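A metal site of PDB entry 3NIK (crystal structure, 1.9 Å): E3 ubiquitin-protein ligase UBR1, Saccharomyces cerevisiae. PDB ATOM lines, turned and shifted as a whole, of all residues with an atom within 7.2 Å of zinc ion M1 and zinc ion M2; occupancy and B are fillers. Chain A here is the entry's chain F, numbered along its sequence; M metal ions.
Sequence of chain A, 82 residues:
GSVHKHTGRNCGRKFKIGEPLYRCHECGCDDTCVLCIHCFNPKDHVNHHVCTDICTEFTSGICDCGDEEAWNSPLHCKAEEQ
Zinc ion M2 is bound by a ring nitrogen (NE2) of His 6 (2.1 Å), the side-chain sulfur (SG) of Cys 65 (2.1 Å), the side-chain sulfur (SG) of Cys 77 (2.3 Å) and the side-chain sulfur (SG) of Cys 39 (2.5 Å).
Within 4 Å of zinc ion M2: His 6, Cys 39, Cys 65 and Cys 77. The nearest printed residue that does not touch zinc ion M2 is Cys 11 (4.4 Å).
Zinc ion M1 is bound by SG of Cys 63 (2.2 Å). The side-chain sulfur (SG) of Cys 11 binds zinc ion M1 (2.3 Å). The side-chain sulfur (SG) of Cys 39 binds zinc ion M1 (2.3 Å). Zinc ion M1 is bound by SG of Cys 36 (2.4 Å). Zinc ion M1 has four donor atoms within binding distance.
ND1 of His 6 sits at hydrogen-bond distance from O of Arg 9, 2.8 Å away. The side-chain sulfur of Cys 63 lies close to the backbone NH of Cys 65 (3.5 Å). The backbone carbonyl oxygen (O) of Cys 65 is in hydrogen-bond range of the backbone NH (N) of Cys 11. The backbone NH of Cys 63 sits at hydrogen-bond distance from the backbone carbonyl oxygen of Arg 13, 3.0 Å away. The backbone NH of Gly 12 is in hydrogen-bond range of the backbone carbonyl oxygen of Cys 63 (2.9 Å). SG of Cys 11 sits close to N of Arg 13. O of Cys 11 is in hydrogen-bond range of NH2 of Arg 9 (3.2 Å). The backbone NH (N) of His 38 lies close to the side-chain sulfur (SG) of Cys 36.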
ATOM      1  N   HIS A   4       3.183 -25.879  29.344  1.00  0.00           N
ATOM      2  CA  HIS A   4       2.313 -26.405  28.302  1.00  0.00           C
ATOM      3  C   HIS A   4       2.179 -25.462  27.103  1.00  0.00           C
ATOM      4  O   HIS A   4       1.383 -25.703  26.181  1.00  0.00           O
ATOM      5  CB  HIS A   4       0.932 -26.731  28.885  1.00  0.00           C
ATOM      6  CG  HIS A   4       0.934 -27.880  29.848  1.00  0.00           C
ATOM      7  ND1 HIS A   4       1.220 -29.173  29.464  1.00  0.00           N
ATOM      8  CD2 HIS A   4       0.688 -27.930  31.175  1.00  0.00           C
ATOM      9  CE1 HIS A   4       1.155 -29.969  30.522  1.00  0.00           C
ATOM     10  NE2 HIS A   4       0.829 -29.236  31.568  1.00  0.00           N
ATOM     11  N   LYS A   5       2.965 -24.386  27.109  1.00  0.00           N
ATOM     12  CA  LYS A   5       2.991 -23.419  26.001  1.00  0.00           C
ATOM     13  C   LYS A   5       3.357 -24.060  24.654  1.00  0.00           C
ATOM     14  O   LYS A   5       4.196 -24.963  24.595  1.00  0.00           O
ATOM     15  CB  LYS A   5       3.936 -22.252  26.300  1.00  0.00           C
ATOM     16  CG  LYS A   5       3.376 -21.211  27.246  1.00  0.00           C
ATOM     17  CD  LYS A   5       4.424 -20.145  27.560  1.00  0.00           C
ATOM     18  CE  LYS A   5       3.911 -19.110  28.541  1.00  0.00           C
ATOM     19  NZ  LYS A   5       4.944 -18.080  28.880  1.00  0.00           N
ATOM     20  N   HIS A   6       2.706 -23.583  23.593  1.00  0.00           N
ATOM     21  CA  HIS A   6       2.931 -24.086  22.233  1.00  0.00           C
ATOM     22  C   HIS A   6       2.850 -22.942  21.221  1.00  0.00           C
ATOM     23  O   HIS A   6       2.469 -23.170  20.069  1.00  0.00           O
ATOM     24  CB  HIS A   6       1.892 -25.153  21.868  1.00  0.00           C
ATOM     25  CG  HIS A   6       0.484 -24.671  21.929  1.00  0.00           C
ATOM     26  ND1 HIS A   6      -0.136 -24.040  20.874  1.00  0.00           N
ATOM     27  CD2 HIS A   6      -0.438 -24.736  22.922  1.00  0.00           C
ATOM     28  CE1 HIS A   6      -1.378 -23.731  21.214  1.00  0.00           C
ATOM     29  NE2 HIS A   6      -1.584 -24.144  22.455  1.00  0.00           N
ATOM     30  N   THR A   7       3.214 -21.743  21.656  1.00  0.00           N
ATOM     31  CA  THR A   7       3.137 -20.549  20.814  1.00  0.00           C
ATOM     32  C   THR A   7       3.947 -20.732  19.527  1.00  0.00           C
ATOM     33  O   THR A   7       5.097 -21.178  19.574  1.00  0.00           O
ATOM     34  CB  THR A   7       3.670 -19.322  21.557  1.00  0.00           C
ATOM     35  OG1 THR A   7       3.277 -19.375  22.924  1.00  0.00           O
ATOM     36  CG2 THR A   7       3.138 -18.040  20.915  1.00  0.00           C
ATOM     37  N   ARG A   9       2.675 -22.683  17.122  1.00  0.00           N
ATOM     38  CA  ARG A   9       2.134 -23.923  16.576  1.00  0.00           C
ATOM     39  C   ARG A   9       0.824 -24.329  17.249  1.00  0.00           C
ATOM     40  O   ARG A   9       0.302 -23.615  18.120  1.00  0.00           O
ATOM     41  CB  ARG A   9       3.166 -25.060  16.665  1.00  0.00           C
ATOM     42  CG  ARG A   9       3.766 -25.245  18.029  1.00  0.00           C
ATOM     43  CD  ARG A   9       4.371 -26.617  18.181  1.00  0.00           C
ATOM     44  NE  ARG A   9       3.338 -27.621  18.411  1.00  0.00           N
ATOM     45  CZ  ARG A   9       3.578 -28.857  18.809  1.00  0.00           C
ATOM     46  NH1 ARG A   9       4.832 -29.268  19.020  1.00  0.00           N
ATOM     47  NH2 ARG A   9       2.554 -29.691  19.002  1.00  0.00           N
ATOM     48  N   ASN A  10       0.296 -25.471  16.823  1.00  0.00           N
ATOM     49  CA  ASN A  10      -0.893 -26.065  17.407  1.00  0.00           C
ATOM     50  C   ASN A  10      -0.537 -26.776  18.697  1.00  0.00           C
ATOM     51  O   ASN A  10       0.619 -27.098  18.951  1.00  0.00           O
ATOM     52  CB  ASN A  10      -1.512 -27.078  16.436  1.00  0.00           C
ATOM     53  CG  ASN A  10      -0.620 -28.267  16.198  1.00  0.00           C
ATOM     54  OD1 ASN A  10       0.556 -28.106  15.867  1.00  0.00           O
ATOM     55  ND2 ASN A  10      -1.160 -29.476  16.378  1.00  0.00           N
ATOM     56  N   CYS A  11      -1.542 -27.016  19.524  1.00  0.00           N
ATOM     57  CA  CYS A  11      -1.308 -27.774  20.753  1.00  0.00           C
ATOM     58  C   CYS A  11      -1.119 -29.242  20.408  1.00  0.00           C
ATOM     59  O   CYS A  11      -0.079 -29.824  20.733  1.00  0.00           O
ATOM     60  CB  CYS A  11      -2.471 -27.620  21.732  1.00  0.00           C
ATOM     61  SG  CYS A  11      -2.269 -28.709  23.140  1.00  0.00           S
ATOM     62  N   GLY A  12      -2.120 -29.838  19.779  1.00  0.00           N
ATOM     63  CA  GLY A  12      -2.057 -31.221  19.295  1.00  0.00           C
ATOM     64  C   GLY A  12      -1.946 -32.323  20.345  1.00  0.00           C
ATOM     65  O   GLY A  12      -1.601 -33.458  20.005  1.00  0.00           O
ATOM     66  N   ARG A  13      -2.253 -32.006  21.605  1.00  0.00           N
ATOM     67  CA  ARG A  13      -2.168 -32.991  22.656  1.00  0.00           C
ATOM     68  C   ARG A  13      -3.160 -34.132  22.413  1.00  0.00           C
ATOM     69  O   ARG A  13      -4.349 -33.899  22.186  1.00  0.00           O
ATOM     70  CB  ARG A  13      -2.427 -32.370  24.034  1.00  0.00           C
ATOM     71  CG  ARG A  13      -2.644 -33.418  25.135  1.00  0.00           C
ATOM     72  CD  ARG A  13      -2.963 -32.813  26.495  1.00  0.00           C
ATOM     73  NE  ARG A  13      -1.802 -32.163  27.091  1.00  0.00           N
ATOM     74  CZ  ARG A  13      -0.904 -32.771  27.870  1.00  0.00           C
ATOM     75  NH1 ARG A  13      -1.016 -34.049  28.171  1.00  0.00           N
ATOM     76  NH2 ARG A  13       0.107 -32.067  28.349  1.00  0.00           N
ATOM     77  N   PHE A  15      -5.368 -36.787  23.974  1.00  0.00           N
ATOM     78  CA  PHE A  15      -6.008 -37.017  25.282  1.00  0.00           C
ATOM     79  C   PHE A  15      -5.763 -38.447  25.791  1.00  0.00           C
ATOM     80  O   PHE A  15      -5.775 -39.396  25.009  1.00  0.00           O
ATOM     81  CB  PHE A  15      -7.518 -36.755  25.165  1.00  0.00           C
ATOM     82  CG  PHE A  15      -7.850 -35.362  24.714  1.00  0.00           C
ATOM     83  CD1 PHE A  15      -7.932 -34.311  25.640  1.00  0.00           C
ATOM     84  CD2 PHE A  15      -8.082 -35.080  23.366  1.00  0.00           C
ATOM     85  CE1 PHE A  15      -8.238 -33.006  25.211  1.00  0.00           C
ATOM     86  CE2 PHE A  15      -8.376 -33.781  22.931  1.00  0.00           C
ATOM     87  CZ  PHE A  15      -8.461 -32.744  23.867  1.00  0.00           C
ATOM     88  N   VAL A  34     -11.810 -29.204  19.407  1.00  0.00           N
ATOM     89  CA  VAL A  34     -11.702 -29.469  20.839  1.00  0.00           C
ATOM     90  C   VAL A  34     -10.520 -28.756  21.503  1.00  0.00           C
ATOM     91  O   VAL A  34      -9.533 -28.398  20.837  1.00  0.00           O
ATOM     92  CB  VAL A  34     -11.620 -30.992  21.176  1.00  0.00           C
ATOM     93  CG1 VAL A  34     -12.836 -31.760  20.662  1.00  0.00           C
ATOM     94  CG2 VAL A  34     -10.322 -31.608  20.669  1.00  0.00           C
ATOM     95  N   LEU A  35     -10.627 -28.569  22.815  1.00  0.00           N
ATOM     96  CA  LEU A  35      -9.580 -27.966  23.622  1.00  0.00           C
ATOM     97  C   LEU A  35      -9.276 -28.830  24.839  1.00  0.00           C
ATOM     98  O   LEU A  35     -10.188 -29.366  25.472  1.00  0.00           O
ATOM     99  CB  LEU A  35      -9.996 -26.572  24.077  1.00  0.00           C
ATOM    100  CG  LEU A  35     -10.092 -25.512  22.977  1.00  0.00           C
ATOM    101  CD1 LEU A  35     -10.865 -24.290  23.465  1.00  0.00           C
ATOM    102  CD2 LEU A  35      -8.685 -25.135  22.519  1.00  0.00           C
ATOM    103  N   CYS A  36      -7.986 -28.961  25.151  1.00  0.00           N
ATOM    104  CA  CYS A  36      -7.529 -29.627  26.369  1.00  0.00           C
ATOM    105  C   CYS A  36      -7.600 -28.683  27.578  1.00  0.00           C
ATOM    106  O   CYS A  36      -7.736 -27.452  27.421  1.00  0.00           O
ATOM    107  CB  CYS A  36      -6.103 -30.168  26.194  1.00  0.00           C
ATOM    108  SG  CYS A  36      -4.762 -28.936  26.366  1.00  0.00           S
ATOM    109  N   ILE A  37      -7.486 -29.272  28.773  1.00  0.00           N
ATOM    110  CA  ILE A  37      -7.538 -28.523  30.033  1.00  0.00           C
ATOM    111  C   ILE A  37      -6.435 -27.479  30.195  1.00  0.00           C
ATOM    112  O   ILE A  37      -6.605 -26.470  30.910  1.00  0.00           O
ATOM    113  CB  ILE A  37      -7.520 -29.457  31.285  1.00  0.00           C
ATOM    114  CG1 ILE A  37      -6.223 -30.275  31.354  1.00  0.00           C
ATOM    115  CG2 ILE A  37      -8.739 -30.353  31.280  1.00  0.00           C
ATOM    116  CD1 ILE A  37      -6.041 -31.086  32.657  1.00  0.00           C
ATOM    117  N   HIS A  38      -5.299 -27.707  29.547  1.00  0.00           N
ATOM    118  CA  HIS A  38      -4.171 -26.797  29.653  1.00  0.00           C
ATOM    119  C   HIS A  38      -4.353 -25.576  28.759  1.00  0.00           C
ATOM    120  O   HIS A  38      -3.682 -24.555  28.963  1.00  0.00           O
ATOM    121  CB  HIS A  38      -2.855 -27.524  29.320  1.00  0.00           C
ATOM    122  CG  HIS A  38      -2.687 -28.810  30.071  1.00  0.00           C
ATOM    123  ND1 HIS A  38      -2.906 -30.041  29.484  1.00  0.00           N
ATOM    124  CD2 HIS A  38      -2.386 -29.058  31.365  1.00  0.00           C
ATOM    125  CE1 HIS A  38      -2.707 -30.989  30.391  1.00  0.00           C
ATOM    126  NE2 HIS A  38      -2.392 -30.421  31.527  1.00  0.00           N
ATOM    127  N   CYS A  39      -5.255 -25.689  27.786  1.00  0.00           N
ATOM    128  CA  CYS A  39      -5.445 -24.630  26.796  1.00  0.00           C
ATOM    129  C   CYS A  39      -6.740 -23.851  26.973  1.00  0.00           C
ATOM    130  O   CYS A  39      -6.754 -22.642  26.754  1.00  0.00           O
ATOM    131  CB  CYS A  39      -5.405 -25.202  25.378  1.00  0.00           C
ATOM    132  SG  CYS A  39      -3.816 -25.857  24.925  1.00  0.00           S
ATOM    133  N   PHE A  40      -7.808 -24.546  27.359  1.00  0.00           N
ATOM    134  CA  PHE A  40      -9.126 -23.935  27.488  1.00  0.00           C
ATOM    135  C   PHE A  40      -9.069 -22.745  28.430  1.00  0.00           C
ATOM    136  O   PHE A  40      -8.694 -22.896  29.595  1.00  0.00           O
ATOM    137  CB  PHE A  40     -10.119 -24.971  28.016  1.00  0.00           C
ATOM    138  CG  PHE A  40     -11.514 -24.440  28.196  1.00  0.00           C
ATOM    139  CD1 PHE A  40     -12.390 -24.369  27.117  1.00  0.00           C
ATOM    140  CD2 PHE A  40     -11.959 -24.012  29.445  1.00  0.00           C
ATOM    141  CE1 PHE A  40     -13.694 -23.870  27.284  1.00  0.00           C
ATOM    142  CE2 PHE A  40     -13.254 -23.533  29.616  1.00  0.00           C
ATOM    143  CZ  PHE A  40     -14.110 -23.446  28.525  1.00  0.00           C
ATOM    144  N   ILE A  62      -7.308 -34.550  18.815  1.00  0.00           N
ATOM    145  CA  ILE A  62      -6.256 -33.928  19.558  1.00  0.00           C
ATOM    146  C   ILE A  62      -6.698 -32.504  19.767  1.00  0.00           C
ATOM    147  O   ILE A  62      -7.529 -31.986  19.008  1.00  0.00           O
ATOM    148  CB  ILE A  62      -4.934 -33.961  18.750  1.00  0.00           C
ATOM    149  CG1 ILE A  62      -5.106 -33.200  17.429  1.00  0.00           C
ATOM    150  CG2 ILE A  62      -4.483 -35.414  18.500  1.00  0.00           C
ATOM    151  CD1 ILE A  62      -3.819 -32.833  16.733  1.00  0.00           C
ATOM    152  N   CYS A  63      -6.123 -31.867  20.776  1.00  0.00           N
ATOM    153  CA  CYS A  63      -6.387 -30.461  21.050  1.00  0.00           C
ATOM    154  C   CYS A  63      -6.084 -29.585  19.843  1.00  0.00           C
ATOM    155  O   CYS A  63      -5.009 -29.697  19.235  1.00  0.00           O
ATOM    156  CB  CYS A  63      -5.560 -30.011  22.248  1.00  0.00           C
ATOM    157  SG  CYS A  63      -5.853 -28.301  22.714  1.00  0.00           S
ATOM    158  N   ASP A  64      -7.035 -28.720  19.512  1.00  0.00           N
ATOM    159  CA  ASP A  64      -6.969 -27.814  18.355  1.00  0.00           C
ATOM    160  C   ASP A  64      -6.539 -26.391  18.671  1.00  0.00           C
ATOM    161  O   ASP A  64      -6.577 -25.514  17.798  1.00  0.00           O
ATOM    162  CB  ASP A  64      -8.343 -27.753  17.688  1.00  0.00           C
ATOM    163  CG  ASP A  64      -8.704 -29.035  16.985  1.00  0.00           C
ATOM    164  OD1 ASP A  64      -7.976 -29.427  16.055  1.00  0.00           O
ATOM    165  OD2 ASP A  64      -9.724 -29.638  17.374  1.00  0.00           O
ATOM    166  N   CYS A  65      -6.145 -26.143  19.919  1.00  0.00           N
ATOM    167  CA  CYS A  65      -5.663 -24.810  20.315  1.00  0.00           C
ATOM    168  C   CYS A  65      -4.493 -24.439  19.405  1.00  0.00           C
ATOM    169  O   CYS A  65      -3.582 -25.239  19.205  1.00  0.00           O
ATOM    170  CB  CYS A  65      -5.226 -24.810  21.792  1.00  0.00           C
ATOM    171  SG  CYS A  65      -4.808 -23.185  22.518  1.00  0.00           S
ATOM    172  N   GLY A  66      -4.547 -23.237  18.820  1.00  0.00           N
ATOM    173  CA  GLY A  66      -3.426 -22.717  18.044  1.00  0.00           C
ATOM    174  C   GLY A  66      -3.492 -23.027  16.556  1.00  0.00           C
ATOM    175  O   GLY A  66      -2.705 -22.500  15.760  1.00  0.00           O
ATOM    176  N   HIS A  76      -7.095 -17.324  23.455  1.00  0.00           N
ATOM    177  CA  HIS A  76      -5.942 -16.972  24.266  1.00  0.00           C
ATOM    178  C   HIS A  76      -5.618 -18.169  25.141  1.00  0.00           C
ATOM    179  O   HIS A  76      -6.213 -18.368  26.205  1.00  0.00           O
ATOM    180  CB  HIS A  76      -6.223 -15.702  25.065  1.00  0.00           C
ATOM    181  CG  HIS A  76      -6.749 -14.593  24.222  1.00  0.00           C
ATOM    182  ND1 HIS A  76      -8.078 -14.505  23.857  1.00  0.00           N
ATOM    183  CD2 HIS A  76      -6.123 -13.565  23.601  1.00  0.00           C
ATOM    184  CE1 HIS A  76      -8.256 -13.456  23.085  1.00  0.00           C
ATOM    185  NE2 HIS A  76      -7.083 -12.867  22.905  1.00  0.00           N
ATOM    186  N   CYS A  77      -4.701 -18.982  24.643  1.00  0.00           N
ATOM    187  CA  CYS A  77      -4.278 -20.220  25.299  1.00  0.00           C
ATOM    188  C   CYS A  77      -4.018 -19.972  26.770  1.00  0.00           C
ATOM    189  O   CYS A  77      -3.295 -19.030  27.134  1.00  0.00           O
ATOM    190  CB  CYS A  77      -3.031 -20.778  24.622  1.00  0.00           C
ATOM    191  SG  CYS A  77      -2.500 -22.319  25.359  1.00  0.00           S
ATOM    192  N   LYS A  78      -4.606 -20.807  27.625  1.00  0.00           N
ATOM    193  CA  LYS A  78      -4.447 -20.644  29.068  1.00  0.00           C
ATOM    194  C   LYS A  78      -2.991 -20.799  29.484  1.00  0.00           C
ATOM    195  O   LYS A  78      -2.532 -20.130  30.414  1.00  0.00           O
ATOM    196  CB  LYS A  78      -5.338 -21.621  29.837  1.00  0.00           C
ATOM    197  CG  LYS A  78      -5.487 -21.239  31.321  1.00  0.00           C
ATOM    198  CD  LYS A  78      -6.472 -22.144  32.034  1.00  0.00           C
ATOM    199  CE  LYS A  78      -6.174 -22.175  33.542  1.00  0.00           C
ATOM    200  NZ  LYS A  78      -4.942 -22.970  33.847  1.00  0.00           N
ATOM    201  N   ALA A  79      -2.246 -21.644  28.766  1.00  0.00           N
ATOM    202  CA  ALA A  79      -0.842 -21.881  29.088  1.00  0.00           C
ATOM    203  C   ALA A  79       0.002 -20.611  28.936  1.00  0.00           C
ATOM    204  O   ALA A  79       1.099 -20.520  29.491  1.00  0.00           O
ATOM    205  CB  ALA A  79      -0.285 -23.005  28.205  1.00  0.00           C
ATOM    206  N   GLU A  80      -0.550 -19.636  28.201  1.00  0.00           N
ATOM    207  CA  GLU A  80       0.146 -18.385  27.887  1.00  0.00           C
ATOM    208  C   GLU A  80      -0.182 -17.263  28.871  1.00  0.00           C
ATOM    209  O   GLU A  80       0.439 -16.188  28.840  1.00  0.00           O
ATOM    210  CB  GLU A  80      -0.146 -17.966  26.444  1.00  0.00           C
ATOM    211  CG  GLU A  80       0.506 -18.892  25.423  1.00  0.00           C
ATOM    212  CD  GLU A  80       0.152 -18.566  23.970  1.00  0.00           C
ATOM    213  OE1 GLU A  80      -0.482 -17.529  23.720  1.00  0.00           O
ATOM    214  OE2 GLU A  80       0.523 -19.372  23.079  1.00  0.00           O
HETATM  215 ZN    ZN M   1      -4.237 -28.059  24.231  1.00  0.00          ZN
HETATM  216 ZN    ZN M   2      -3.190 -23.789  23.754  1.00  0.00          ZN
